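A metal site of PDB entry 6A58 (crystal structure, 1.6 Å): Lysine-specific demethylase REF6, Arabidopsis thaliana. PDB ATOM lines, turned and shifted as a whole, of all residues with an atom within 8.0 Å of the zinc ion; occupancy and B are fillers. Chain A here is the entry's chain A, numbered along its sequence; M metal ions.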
ATOM      1  N   ILE A  47      -1.914  -7.394   6.067  1.00  0.00           N
ATOM      2  CA  ILE A  47      -3.300  -7.825   5.941  1.00  0.00           C
ATOM      3  C   ILE A  47      -3.420  -9.170   6.654  1.00  0.00           C
ATOM      4  O   ILE A  47      -2.590 -10.054   6.440  1.00  0.00           O
ATOM      5  CB  ILE A  47      -3.713  -7.991   4.460  1.00  0.00           C
ATOM      6  CG1 ILE A  47      -3.579  -6.655   3.716  1.00  0.00           C
ATOM      7  CG2 ILE A  47      -5.148  -8.511   4.352  1.00  0.00           C
ATOM      8  CD1 ILE A  47      -3.497  -6.791   2.212  1.00  0.00           C
ATOM      9  N   CYS A  48      -4.433  -9.298   7.501  1.00  0.00           N
ATOM     10  CA  CYS A  48      -4.669 -10.546   8.252  1.00  0.00           C
ATOM     11  C   CYS A  48      -4.636 -11.777   7.338  1.00  0.00           C
ATOM     12  O   CYS A  48      -5.237 -11.748   6.258  1.00  0.00           O
ATOM     13  CB  CYS A  48      -6.010 -10.473   8.980  1.00  0.00           C
ATOM     14  SG  CYS A  48      -6.349 -11.932   9.985  1.00  0.00           S
ATOM     15  N   PRO A  49      -3.967 -12.869   7.769  1.00  0.00           N
ATOM     16  CA  PRO A  49      -3.892 -14.073   6.931  1.00  0.00           C
ATOM     17  C   PRO A  49      -5.149 -14.937   6.881  1.00  0.00           C
ATOM     18  O   PRO A  49      -5.192 -15.887   6.091  1.00  0.00           O
ATOM     19  CB  PRO A  49      -2.756 -14.879   7.583  1.00  0.00           C
ATOM     20  CG  PRO A  49      -2.797 -14.465   9.014  1.00  0.00           C
ATOM     21  CD  PRO A  49      -3.152 -12.999   8.992  1.00  0.00           C
ATOM     22  N   ILE A  50      -6.160 -14.624   7.699  1.00  0.00           N
ATOM     23  CA  ILE A  50      -7.339 -15.489   7.866  1.00  0.00           C
ATOM     24  C   ILE A  50      -8.441 -15.135   6.869  1.00  0.00           C
ATOM     25  O   ILE A  50      -8.794 -13.961   6.701  1.00  0.00           O
ATOM     26  CB  ILE A  50      -7.886 -15.410   9.309  1.00  0.00           C
ATOM     27  CG1 ILE A  50      -6.793 -15.810  10.324  1.00  0.00           C
ATOM     28  CG2 ILE A  50      -9.145 -16.257   9.475  1.00  0.00           C
ATOM     29  CD1 ILE A  50      -6.227 -17.200  10.153  1.00  0.00           C
ATOM     30  N   LYS A  51      -8.992 -16.163   6.221  1.00  0.00           N
ATOM     31  CA  LYS A  51     -10.095 -15.990   5.259  1.00  0.00           C
ATOM     32  C   LYS A  51     -11.288 -15.276   5.910  1.00  0.00           C
ATOM     33  O   LYS A  51     -11.709 -15.622   7.013  1.00  0.00           O
ATOM     34  CB  LYS A  51     -10.552 -17.358   4.722  1.00  0.00           C
ATOM     35  CG  LYS A  51      -9.546 -18.054   3.821  1.00  0.00           C
ATOM     36  CD  LYS A  51      -9.904 -19.514   3.597  1.00  0.00           C
ATOM     37  CE  LYS A  51      -8.883 -20.221   2.739  1.00  0.00           C
ATOM     38  NZ  LYS A  51      -9.168 -21.674   2.551  1.00  0.00           N
ATOM     39  N   GLY A  52     -11.802 -14.259   5.216  1.00  0.00           N
ATOM     40  CA  GLY A  52     -12.975 -13.504   5.673  1.00  0.00           C
ATOM     41  C   GLY A  52     -12.758 -12.340   6.624  1.00  0.00           C
ATOM     42  O   GLY A  52     -13.699 -11.592   6.884  1.00  0.00           O
ATOM     43  N   CYS A  53     -11.543 -12.171   7.147  1.00  0.00           N
ATOM     44  CA  CYS A  53     -11.274 -11.128   8.144  1.00  0.00           C
ATOM     45  C   CYS A  53     -11.109  -9.759   7.469  1.00  0.00           C
ATOM     46  O   CYS A  53     -11.916  -8.857   7.676  1.00  0.00           O
ATOM     47  CB  CYS A  53     -10.053 -11.468   9.000  1.00  0.00           C
ATOM     48  SG  CYS A  53      -9.654 -10.205  10.222  1.00  0.00           S
ATOM     49  N   GLY A  54     -10.042  -9.617   6.681  1.00  0.00           N
ATOM     50  CA  GLY A  54      -9.778  -8.385   5.928  1.00  0.00           C
ATOM     51  C   GLY A  54      -9.155  -7.219   6.689  1.00  0.00           C
ATOM     52  O   GLY A  54      -8.898  -6.172   6.086  1.00  0.00           O
ATOM     53  N   LYS A  55      -8.889  -7.379   7.983  1.00  0.00           N
ATOM     54  CA  LYS A  55      -8.305  -6.296   8.779  1.00  0.00           C
ATOM     55  C   LYS A  55      -6.854  -6.034   8.370  1.00  0.00           C
ATOM     56  O   LYS A  55      -6.094  -6.981   8.156  1.00  0.00           O
ATOM     57  CB  LYS A  55      -8.408  -6.596  10.274  1.00  0.00           C
ATOM     58  CG  LYS A  55      -9.843  -6.622  10.795  1.00  0.00           C
ATOM     59  CD  LYS A  55      -9.865  -6.937  12.279  1.00  0.00           C
ATOM     60  CE  LYS A  55     -11.235  -6.678  12.905  1.00  0.00           C
ATOM     61  NZ  LYS A  55     -12.289  -7.585  12.368  1.00  0.00           N
ATOM     62  N   ASN A  56      -6.506  -4.756   8.233  1.00  0.00           N
ATOM     63  CA  ASN A  56      -5.137  -4.320   7.906  1.00  0.00           C
ATOM     64  C   ASN A  56      -4.544  -3.640   9.127  1.00  0.00           C
ATOM     65  O   ASN A  56      -5.274  -3.024   9.917  1.00  0.00           O
ATOM     66  CB  ASN A  56      -5.136  -3.307   6.757  1.00  0.00           C
ATOM     67  CG  ASN A  56      -5.464  -3.910   5.406  1.00  0.00           C
ATOM     68  OD1 ASN A  56      -4.830  -3.559   4.406  1.00  0.00           O
ATOM     69  ND2 ASN A  56      -6.484  -4.779   5.349  1.00  0.00           N
ATOM     70  N   PHE A  57      -3.218  -3.701   9.271  1.00  0.00           N
ATOM     71  CA  PHE A  57      -2.527  -3.164  10.441  1.00  0.00           C
ATOM     72  C   PHE A  57      -1.348  -2.272  10.083  1.00  0.00           C
ATOM     73  O   PHE A  57      -0.793  -2.356   8.991  1.00  0.00           O
ATOM     74  CB  PHE A  57      -2.112  -4.310  11.366  1.00  0.00           C
ATOM     75  CG  PHE A  57      -3.284  -5.040  11.933  1.00  0.00           C
ATOM     76  CD1 PHE A  57      -3.886  -4.610  13.102  1.00  0.00           C
ATOM     77  CD2 PHE A  57      -3.858  -6.114  11.250  1.00  0.00           C
ATOM     78  CE1 PHE A  57      -5.006  -5.241  13.610  1.00  0.00           C
ATOM     79  CE2 PHE A  57      -4.982  -6.757  11.740  1.00  0.00           C
ATOM     80  CZ  PHE A  57      -5.556  -6.323  12.927  1.00  0.00           C
ATOM     81  N   LEU A  63      -0.064  -7.016  13.374  1.00  0.00           N
ATOM     82  CA  LEU A  63      -0.601  -8.112  12.563  1.00  0.00           C
ATOM     83  C   LEU A  63      -0.478  -9.470  13.269  1.00  0.00           C
ATOM     84  O   LEU A  63      -1.451 -10.222  13.347  1.00  0.00           O
ATOM     85  CB  LEU A  63       0.109  -8.171  11.217  1.00  0.00           C
ATOM     86  CG  LEU A  63      -0.247  -9.322  10.267  1.00  0.00           C
ATOM     87  CD1 LEU A  63      -1.642  -9.126   9.707  1.00  0.00           C
ATOM     88  CD2 LEU A  63       0.804  -9.451   9.169  1.00  0.00           C
ATOM     89  N   HIS A  66      -2.688  -9.853  16.356  1.00  0.00           N
ATOM     90  CA  HIS A  66      -4.089 -10.013  15.940  1.00  0.00           C
ATOM     91  C   HIS A  66      -4.438 -11.434  15.492  1.00  0.00           C
ATOM     92  O   HIS A  66      -5.472 -11.969  15.884  1.00  0.00           O
ATOM     93  CB  HIS A  66      -4.444  -9.034  14.823  1.00  0.00           C
ATOM     94  CG  HIS A  66      -5.796  -9.283  14.227  1.00  0.00           C
ATOM     95  ND1 HIS A  66      -6.960  -8.999  14.896  1.00  0.00           N
ATOM     96  CD2 HIS A  66      -6.156  -9.832  13.040  1.00  0.00           C
ATOM     97  CE1 HIS A  66      -7.991  -9.338  14.139  1.00  0.00           C
ATOM     98  NE2 HIS A  66      -7.538  -9.846  13.012  1.00  0.00           N
ATOM     99  N   GLN A  67      -3.583 -12.025  14.651  1.00  0.00           N
ATOM    100  CA  GLN A  67      -3.797 -13.382  14.112  1.00  0.00           C
ATOM    101  C   GLN A  67      -4.056 -14.420  15.214  1.00  0.00           C
ATOM    102  O   GLN A  67      -4.872 -15.332  15.037  1.00  0.00           O
ATOM    103  CB  GLN A  67      -2.616 -13.806  13.212  1.00  0.00           C
ATOM    104  CG  GLN A  67      -2.617 -15.263  12.744  1.00  0.00           C
ATOM    105  CD  GLN A  67      -1.880 -16.211  13.690  1.00  0.00           C
ATOM    106  OE1 GLN A  67      -0.792 -15.901  14.173  1.00  0.00           O
ATOM    107  NE2 GLN A  67      -2.481 -17.369  13.948  1.00  0.00           N
ATOM    108  N   ARG A  68      -3.373 -14.266  16.353  1.00  0.00           N
ATOM    109  CA  ARG A  68      -3.557 -15.141  17.524  1.00  0.00           C
ATOM    110  C   ARG A  68      -4.993 -15.159  18.068  1.00  0.00           C
ATOM    111  O   ARG A  68      -5.434 -16.184  18.591  1.00  0.00           O
ATOM    112  CB  ARG A  68      -2.599 -14.727  18.638  1.00  0.00           C
ATOM    113  N   VAL A  69      -5.714 -14.041  17.933  1.00  0.00           N
ATOM    114  CA  VAL A  69      -7.117 -13.952  18.368  1.00  0.00           C
ATOM    115  C   VAL A  69      -8.068 -14.875  17.587  1.00  0.00           C
ATOM    116  O   VAL A  69      -9.092 -15.296  18.125  1.00  0.00           O
ATOM    117  CB  VAL A  69      -7.641 -12.503  18.264  1.00  0.00           C
ATOM    118  N   HIS A  70      -7.741 -15.172  16.329  1.00  0.00           N
ATOM    119  CA  HIS A  70      -8.501 -16.144  15.535  1.00  0.00           C
ATOM    120  C   HIS A  70      -8.288 -17.595  15.974  1.00  0.00           C
ATOM    121  O   HIS A  70      -9.179 -18.426  15.812  1.00  0.00           O
ATOM    122  CB  HIS A  70      -8.148 -16.029  14.046  1.00  0.00           C
ATOM    123  CG  HIS A  70      -8.648 -14.776  13.405  1.00  0.00           C
ATOM    124  ND1 HIS A  70      -9.919 -14.673  12.874  1.00  0.00           N
ATOM    125  CD2 HIS A  70      -8.054 -13.579  13.178  1.00  0.00           C
ATOM    126  CE1 HIS A  70     -10.088 -13.462  12.369  1.00  0.00           C
ATOM    127  NE2 HIS A  70      -8.965 -12.779  12.540  1.00  0.00           N
HETATM  128 ZN    ZN M   1      -7.996 -11.227  11.310  1.00  0.00          ZN
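Four residues have an atom within 4 Å of the zinc ion: Cys 48, Cys 53, His 66 and His 70. The nearest printed residue that does not touch the zinc ion is Ile 50 (4.6 Å).
NE2 of His 70 binds the zinc ion. SG of Cys 48 is bound to the zinc ion. The zinc ion is bound by SG of Cys 53, at 2.2 Å. The zinc ion is bound by NE2 of His 66 (2.2 Å). The zinc ion has four donor atoms within binding distance.
SG of Cys 48 lies close to N of Ile 50, 3.5 Å away. N of Cys 48 sits at hydrogen-bond distance from O of Lys 55 (2.9 Å). The side-chain sulfur (SG) of Cys 53 lies close to the backbone NH (N) of Lys 55 (3.7 Å).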
